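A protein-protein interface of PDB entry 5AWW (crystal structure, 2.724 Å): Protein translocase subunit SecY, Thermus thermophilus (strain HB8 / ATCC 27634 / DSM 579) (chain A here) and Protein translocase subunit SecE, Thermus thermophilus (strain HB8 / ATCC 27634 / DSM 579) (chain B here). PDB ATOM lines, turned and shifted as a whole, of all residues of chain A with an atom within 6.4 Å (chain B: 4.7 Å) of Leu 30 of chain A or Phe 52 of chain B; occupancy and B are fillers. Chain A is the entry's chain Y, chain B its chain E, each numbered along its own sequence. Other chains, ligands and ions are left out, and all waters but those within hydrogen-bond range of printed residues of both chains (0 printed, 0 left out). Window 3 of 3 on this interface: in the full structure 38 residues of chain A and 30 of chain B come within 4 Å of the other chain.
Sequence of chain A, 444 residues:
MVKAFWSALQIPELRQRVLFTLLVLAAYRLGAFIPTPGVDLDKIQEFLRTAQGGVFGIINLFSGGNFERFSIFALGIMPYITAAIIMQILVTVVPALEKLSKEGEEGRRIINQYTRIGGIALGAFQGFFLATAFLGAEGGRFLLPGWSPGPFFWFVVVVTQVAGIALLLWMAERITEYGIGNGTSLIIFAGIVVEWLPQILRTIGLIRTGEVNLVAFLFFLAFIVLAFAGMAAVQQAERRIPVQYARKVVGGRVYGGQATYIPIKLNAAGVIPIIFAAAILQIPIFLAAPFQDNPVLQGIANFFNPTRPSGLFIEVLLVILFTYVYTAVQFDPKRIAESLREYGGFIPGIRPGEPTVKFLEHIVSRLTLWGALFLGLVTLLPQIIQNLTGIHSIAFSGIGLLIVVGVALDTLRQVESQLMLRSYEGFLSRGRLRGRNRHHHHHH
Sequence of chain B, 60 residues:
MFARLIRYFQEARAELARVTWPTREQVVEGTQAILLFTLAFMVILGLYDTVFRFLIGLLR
OD2 of Asp 49 of chain B lies within salt-bridge range of NH2 of Arg 29 of chain A (3.8 Å).
The guanidinium group (NH1) of Arg 53 of chain B is in salt-bridge range of the side-chain carboxylate (OD2) of Asp 49 of chain B (2.8 Å).
Ala 26 of chain A touches Tyr 48 of chain B (CB to CZ, 3.6 Å). Ala 26 of chain A touches Phe 52 of chain B (O to CE2, 3.5 Å). Leu 30 of chain A touches Phe 52 of chain B. Arg 53 of chain B touches Phe 33 of chain A (CG to CE1, 3.7 Å). Phe 33 of chain A touches Ile 56 of chain B.
Leu 30 of chain A touches one residue of chain B. Of chain A, only Ala 26 (3.5 Å) and Leu 30 (3.6 Å) come within 4 Å of Phe 52 of chain B. Of the printed residues of chain A, Tyr 48 of chain B touches Ala 26 (3.6 Å). Of the printed residues of chain A, Asp 49 of chain B touches Arg 29 (3.5 Å). Ile 34 of chain A touches none of the printed residues of chain B. Tyr 28 of chain A touches none of the printed residues of chain B. The nearest printed residue of chain B that does not touch Leu 30 of chain A is Ile 56 of chain B (5.5 Å).
Printed residues of chain A that touch a printed residue of chain B: Ala 26, Arg 29, Leu 30 and Phe 33. Of the 10 printed residues of chain B, 5 touch a printed residue of chain A. Hydrophobic or aromatic side chains of chain B within 4 Å of the printed part of chain A: Tyr 48, Phe 52 and Ile 56. Among the printed residues, Asp or Glu carboxylates within 4 Å of a Lys or Arg side-chain nitrogen of the other chain: Arg 29 of chain A with Asp 49 of chain B (3.8 Å).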
ATOM      1  N   LEU A  25     -26.713   0.141  14.368  1.00  0.00           N
ATOM      2  CA  LEU A  25     -26.139   0.338  15.696  1.00  0.00           C
ATOM      3  C   LEU A  25     -26.627  -0.737  16.662  1.00  0.00           C
ATOM      4  O   LEU A  25     -25.903  -1.140  17.577  1.00  0.00           O
ATOM      5  CB  LEU A  25     -26.477   1.730  16.234  1.00  0.00           C
ATOM      6  CG  LEU A  25     -25.776   2.909  15.557  1.00  0.00           C
ATOM      7  CD1 LEU A  25     -26.202   4.222  16.195  1.00  0.00           C
ATOM      8  CD2 LEU A  25     -24.262   2.747  15.616  1.00  0.00           C
ATOM      9  N   ALA A  26     -27.854  -1.201  16.450  1.00  0.00           N
ATOM     10  CA  ALA A  26     -28.392  -2.314  17.222  1.00  0.00           C
ATOM     11  C   ALA A  26     -27.609  -3.582  16.920  1.00  0.00           C
ATOM     12  O   ALA A  26     -27.311  -4.363  17.821  1.00  0.00           O
ATOM     13  CB  ALA A  26     -29.866  -2.516  16.921  1.00  0.00           C
ATOM     14  N   ALA A  27     -27.277  -3.782  15.648  1.00  0.00           N
ATOM     15  CA  ALA A  27     -26.496  -4.947  15.241  1.00  0.00           C
ATOM     16  C   ALA A  27     -25.095  -4.907  15.843  1.00  0.00           C
ATOM     17  O   ALA A  27     -24.541  -5.937  16.215  1.00  0.00           O
ATOM     18  CB  ALA A  27     -26.418  -5.033  13.726  1.00  0.00           C
ATOM     19  N   TYR A  28     -24.530  -3.708  15.933  1.00  0.00           N
ATOM     20  CA  TYR A  28     -23.212  -3.503  16.525  1.00  0.00           C
ATOM     21  C   TYR A  28     -23.224  -3.808  18.023  1.00  0.00           C
ATOM     22  O   TYR A  28     -22.407  -4.593  18.525  1.00  0.00           O
ATOM     23  CB  TYR A  28     -22.749  -2.066  16.271  1.00  0.00           C
ATOM     24  CG  TYR A  28     -21.469  -1.676  16.970  1.00  0.00           C
ATOM     25  CD1 TYR A  28     -20.313  -2.427  16.815  1.00  0.00           C
ATOM     26  CD2 TYR A  28     -21.411  -0.540  17.768  1.00  0.00           C
ATOM     27  CE1 TYR A  28     -19.137  -2.067  17.448  1.00  0.00           C
ATOM     28  CE2 TYR A  28     -20.242  -0.172  18.403  1.00  0.00           C
ATOM     29  CZ  TYR A  28     -19.108  -0.939  18.240  1.00  0.00           C
ATOM     30  OH  TYR A  28     -17.943  -0.575  18.871  1.00  0.00           O
ATOM     31  N   ARG A  29     -24.163  -3.185  18.729  1.00  0.00           N
ATOM     32  CA  ARG A  29     -24.322  -3.403  20.159  1.00  0.00           C
ATOM     33  C   ARG A  29     -24.573  -4.875  20.465  1.00  0.00           C
ATOM     34  O   ARG A  29     -24.042  -5.415  21.433  1.00  0.00           O
ATOM     35  CB  ARG A  29     -25.465  -2.546  20.707  1.00  0.00           C
ATOM     36  CG  ARG A  29     -25.626  -2.636  22.214  1.00  0.00           C
ATOM     37  CD  ARG A  29     -24.306  -2.372  22.918  1.00  0.00           C
ATOM     38  NE  ARG A  29     -24.463  -2.327  24.368  1.00  0.00           N
ATOM     39  CZ  ARG A  29     -23.461  -2.150  25.222  1.00  0.00           C
ATOM     40  NH1 ARG A  29     -22.221  -2.004  24.773  1.00  0.00           N
ATOM     41  NH2 ARG A  29     -23.699  -2.123  26.526  1.00  0.00           N
ATOM     42  N   LEU A  30     -25.388  -5.521  19.636  1.00  0.00           N
ATOM     43  CA  LEU A  30     -25.627  -6.952  19.767  1.00  0.00           C
ATOM     44  C   LEU A  30     -24.331  -7.717  19.544  1.00  0.00           C
ATOM     45  O   LEU A  30     -24.046  -8.698  20.229  1.00  0.00           O
ATOM     46  CB  LEU A  30     -26.693  -7.419  18.774  1.00  0.00           C
ATOM     47  CG  LEU A  30     -26.989  -8.921  18.766  1.00  0.00           C
ATOM     48  CD1 LEU A  30     -27.496  -9.373  20.128  1.00  0.00           C
ATOM     49  CD2 LEU A  30     -27.987  -9.269  17.674  1.00  0.00           C
ATOM     50  N   GLY A  31     -23.545  -7.244  18.582  1.00  0.00           N
ATOM     51  CA  GLY A  31     -22.279  -7.861  18.245  1.00  0.00           C
ATOM     52  C   GLY A  31     -21.297  -7.763  19.388  1.00  0.00           C
ATOM     53  O   GLY A  31     -20.340  -8.533  19.467  1.00  0.00           O
ATOM     54  N   ALA A  32     -21.536  -6.811  20.284  1.00  0.00           N
ATOM     55  CA  ALA A  32     -20.701  -6.664  21.474  1.00  0.00           C
ATOM     56  C   ALA A  32     -20.879  -7.821  22.462  1.00  0.00           C
ATOM     57  O   ALA A  32     -20.059  -8.002  23.361  1.00  0.00           O
ATOM     58  CB  ALA A  32     -20.995  -5.341  22.162  1.00  0.00           C
ATOM     59  N   PHE A  33     -21.941  -8.604  22.295  1.00  0.00           N
ATOM     60  CA  PHE A  33     -22.228  -9.703  23.216  1.00  0.00           C
ATOM     61  C   PHE A  33     -21.791 -11.061  22.667  1.00  0.00           C
ATOM     62  O   PHE A  33     -22.084 -12.101  23.255  1.00  0.00           O
ATOM     63  CB  PHE A  33     -23.719  -9.738  23.555  1.00  0.00           C
ATOM     64  CG  PHE A  33     -24.183  -8.557  24.359  1.00  0.00           C
ATOM     65  CD1 PHE A  33     -24.143  -8.583  25.742  1.00  0.00           C
ATOM     66  CD2 PHE A  33     -24.660  -7.418  23.731  1.00  0.00           C
ATOM     67  CE1 PHE A  33     -24.569  -7.496  26.484  1.00  0.00           C
ATOM     68  CE2 PHE A  33     -25.086  -6.329  24.466  1.00  0.00           C
ATOM     69  CZ  PHE A  33     -25.041  -6.368  25.844  1.00  0.00           C
ATOM     70  N   ILE A  34     -21.084 -11.046  21.543  1.00  0.00           N
ATOM     71  CA  ILE A  34     -20.575 -12.276  20.949  1.00  0.00           C
ATOM     72  C   ILE A  34     -19.070 -12.380  21.180  1.00  0.00           C
ATOM     73  O   ILE A  34     -18.285 -11.716  20.504  1.00  0.00           O
ATOM     74  CB  ILE A  34     -20.889 -12.343  19.447  1.00  0.00           C
ATOM     75  CG1 ILE A  34     -22.395 -12.205  19.233  1.00  0.00           C
ATOM     76  CG2 ILE A  34     -20.381 -13.648  18.847  1.00  0.00           C
ATOM     77  CD1 ILE A  34     -22.789 -12.007  17.803  1.00  0.00           C
ATOM     78  N   PHE A  73     -15.722  -7.648  17.387  1.00  0.00           N
ATOM     79  CA  PHE A  73     -15.022  -6.395  17.134  1.00  0.00           C
ATOM     80  C   PHE A  73     -14.337  -5.944  18.412  1.00  0.00           C
ATOM     81  O   PHE A  73     -14.737  -4.945  19.004  1.00  0.00           O
ATOM     82  CB  PHE A  73     -15.967  -5.288  16.652  1.00  0.00           C
ATOM     83  CG  PHE A  73     -17.267  -5.781  16.087  1.00  0.00           C
ATOM     84  CD1 PHE A  73     -17.350  -6.206  14.772  1.00  0.00           C
ATOM     85  CD2 PHE A  73     -18.418  -5.778  16.861  1.00  0.00           C
ATOM     86  CE1 PHE A  73     -18.551  -6.643  14.242  1.00  0.00           C
ATOM     87  CE2 PHE A  73     -19.622  -6.213  16.339  1.00  0.00           C
ATOM     88  CZ  PHE A  73     -19.688  -6.647  15.024  1.00  0.00           C
ATOM     89  N   LEU B  47     -32.328   0.931  25.676  1.00  0.00           N
ATOM     90  CA  LEU B  47     -33.300  -0.111  25.375  1.00  0.00           C
ATOM     91  C   LEU B  47     -32.629  -1.287  24.672  1.00  0.00           C
ATOM     92  O   LEU B  47     -32.966  -2.440  24.934  1.00  0.00           O
ATOM     93  CB  LEU B  47     -34.439   0.436  24.513  1.00  0.00           C
ATOM     94  CG  LEU B  47     -35.411   1.399  25.195  1.00  0.00           C
ATOM     95  CD1 LEU B  47     -36.439   1.910  24.198  1.00  0.00           C
ATOM     96  CD2 LEU B  47     -36.095   0.725  26.373  1.00  0.00           C
ATOM     97  N   TYR B  48     -31.683  -0.993  23.784  1.00  0.00           N
ATOM     98  CA  TYR B  48     -30.953  -2.051  23.092  1.00  0.00           C
ATOM     99  C   TYR B  48     -30.285  -3.005  24.074  1.00  0.00           C
ATOM    100  O   TYR B  48     -30.634  -4.181  24.125  1.00  0.00           O
ATOM    101  CB  TYR B  48     -29.896  -1.475  22.150  1.00  0.00           C
ATOM    102  CG  TYR B  48     -30.450  -0.879  20.881  1.00  0.00           C
ATOM    103  CD1 TYR B  48     -31.769  -1.092  20.505  1.00  0.00           C
ATOM    104  CD2 TYR B  48     -29.649  -0.104  20.053  1.00  0.00           C
ATOM    105  CE1 TYR B  48     -32.275  -0.544  19.342  1.00  0.00           C
ATOM    106  CE2 TYR B  48     -30.144   0.448  18.893  1.00  0.00           C
ATOM    107  CZ  TYR B  48     -31.457   0.226  18.540  1.00  0.00           C
ATOM    108  OH  TYR B  48     -31.950   0.775  17.381  1.00  0.00           O
ATOM    109  N   ASP B  49     -29.336  -2.505  24.862  1.00  0.00           N
ATOM    110  CA  ASP B  49     -28.584  -3.397  25.742  1.00  0.00           C
ATOM    111  C   ASP B  49     -29.452  -3.922  26.892  1.00  0.00           C
ATOM    112  O   ASP B  49     -29.149  -4.969  27.474  1.00  0.00           O
ATOM    113  CB  ASP B  49     -27.323  -2.708  26.281  1.00  0.00           C
ATOM    114  CG  ASP B  49     -27.620  -1.674  27.346  1.00  0.00           C
ATOM    115  OD1 ASP B  49     -28.526  -0.846  27.139  1.00  0.00           O
ATOM    116  OD2 ASP B  49     -26.937  -1.689  28.391  1.00  0.00           O
ATOM    117  N   THR B  50     -30.538  -3.217  27.201  1.00  0.00           N
ATOM    118  CA  THR B  50     -31.491  -3.707  28.196  1.00  0.00           C
ATOM    119  C   THR B  50     -32.194  -4.964  27.694  1.00  0.00           C
ATOM    120  O   THR B  50     -32.113  -6.019  28.320  1.00  0.00           O
ATOM    121  CB  THR B  50     -32.554  -2.650  28.557  1.00  0.00           C
ATOM    122  OG1 THR B  50     -31.917  -1.507  29.139  1.00  0.00           O
ATOM    123  CG2 THR B  50     -33.560  -3.221  29.546  1.00  0.00           C
ATOM    124  N   VAL B  51     -32.878  -4.843  26.560  1.00  0.00           N
ATOM    125  CA  VAL B  51     -33.566  -5.971  25.941  1.00  0.00           C
ATOM    126  C   VAL B  51     -32.597  -7.117  25.637  1.00  0.00           C
ATOM    127  O   VAL B  51     -32.919  -8.288  25.854  1.00  0.00           O
ATOM    128  CB  VAL B  51     -34.282  -5.538  24.638  1.00  0.00           C
ATOM    129  CG1 VAL B  51     -34.817  -6.745  23.881  1.00  0.00           C
ATOM    130  CG2 VAL B  51     -35.405  -4.560  24.951  1.00  0.00           C
ATOM    131  N   PHE B  52     -31.407  -6.771  25.155  1.00  0.00           N
ATOM    132  CA  PHE B  52     -30.388  -7.766  24.836  1.00  0.00           C
ATOM    133  C   PHE B  52     -29.974  -8.562  26.068  1.00  0.00           C
ATOM    134  O   PHE B  52     -30.039  -9.792  26.069  1.00  0.00           O
ATOM    135  CB  PHE B  52     -29.156  -7.105  24.213  1.00  0.00           C
ATOM    136  CG  PHE B  52     -29.368  -6.635  22.801  1.00  0.00           C
ATOM    137  CD1 PHE B  52     -30.425  -7.115  22.046  1.00  0.00           C
ATOM    138  CD2 PHE B  52     -28.505  -5.713  22.229  1.00  0.00           C
ATOM    139  CE1 PHE B  52     -30.622  -6.683  20.748  1.00  0.00           C
ATOM    140  CE2 PHE B  52     -28.694  -5.276  20.932  1.00  0.00           C
ATOM    141  CZ  PHE B  52     -29.755  -5.763  20.190  1.00  0.00           C
ATOM    142  N   ARG B  53     -29.556  -7.867  27.121  1.00  0.00           N
ATOM    143  CA  ARG B  53     -29.105  -8.562  28.324  1.00  0.00           C
ATOM    144  C   ARG B  53     -30.251  -9.280  29.037  1.00  0.00           C
ATOM    145  O   ARG B  53     -30.023 -10.252  29.758  1.00  0.00           O
ATOM    146  CB  ARG B  53     -28.410  -7.594  29.284  1.00  0.00           C
ATOM    147  CG  ARG B  53     -26.898  -7.767  29.308  1.00  0.00           C
ATOM    148  CD  ARG B  53     -26.239  -6.914  30.378  1.00  0.00           C
ATOM    149  NE  ARG B  53     -26.233  -5.495  30.033  1.00  0.00           N
ATOM    150  CZ  ARG B  53     -25.637  -4.556  30.758  1.00  0.00           C
ATOM    151  NH1 ARG B  53     -25.680  -3.288  30.370  1.00  0.00           N
ATOM    152  NH2 ARG B  53     -24.996  -4.884  31.872  1.00  0.00           N
ATOM    153  N   PHE B  54     -31.478  -8.812  28.833  1.00  0.00           N
ATOM    154  CA  PHE B  54     -32.637  -9.473  29.428  1.00  0.00           C
ATOM    155  C   PHE B  54     -32.950 -10.780  28.697  1.00  0.00           C
ATOM    156  O   PHE B  54     -33.295 -11.780  29.327  1.00  0.00           O
ATOM    157  CB  PHE B  54     -33.856  -8.544  29.421  1.00  0.00           C
ATOM    158  CG  PHE B  54     -34.031  -7.751  30.698  1.00  0.00           C
ATOM    159  CD1 PHE B  54     -33.120  -6.767  31.057  1.00  0.00           C
ATOM    160  CD2 PHE B  54     -35.117  -7.982  31.530  1.00  0.00           C
ATOM    161  CE1 PHE B  54     -33.284  -6.037  32.225  1.00  0.00           C
ATOM    162  CE2 PHE B  54     -35.287  -7.254  32.698  1.00  0.00           C
ATOM    163  CZ  PHE B  54     -34.369  -6.281  33.045  1.00  0.00           C
ATOM    164  N   LEU B  55     -32.819 -10.775  27.372  1.00  0.00           N
ATOM    165  CA  LEU B  55     -33.045 -11.983  26.575  1.00  0.00           C
ATOM    166  C   LEU B  55     -31.931 -13.012  26.782  1.00  0.00           C
ATOM    167  O   LEU B  55     -32.194 -14.211  26.911  1.00  0.00           O
ATOM    168  CB  LEU B  55     -33.167 -11.635  25.090  1.00  0.00           C
ATOM    169  CG  LEU B  55     -34.442 -10.911  24.651  1.00  0.00           C
ATOM    170  CD1 LEU B  55     -34.429 -10.646  23.151  1.00  0.00           C
ATOM    171  CD2 LEU B  55     -35.674 -11.710  25.043  1.00  0.00           C
ATOM    172  N   ILE B  56     -30.688 -12.538  26.809  1.00  0.00           N
ATOM    173  CA  ILE B  56     -29.544 -13.407  27.070  1.00  0.00           C
ATOM    174  C   ILE B  56     -29.616 -13.970  28.489  1.00  0.00           C
ATOM    175  O   ILE B  56     -29.300 -15.138  28.722  1.00  0.00           O
ATOM    176  CB  ILE B  56     -28.207 -12.662  26.871  1.00  0.00           C
ATOM    177  CG1 ILE B  56     -28.045 -12.241  25.410  1.00  0.00           C
ATOM    178  CG2 ILE B  56     -27.033 -13.532  27.290  1.00  0.00           C
ATOM    179  CD1 ILE B  56     -26.769 -11.478  25.135  1.00  0.00           C
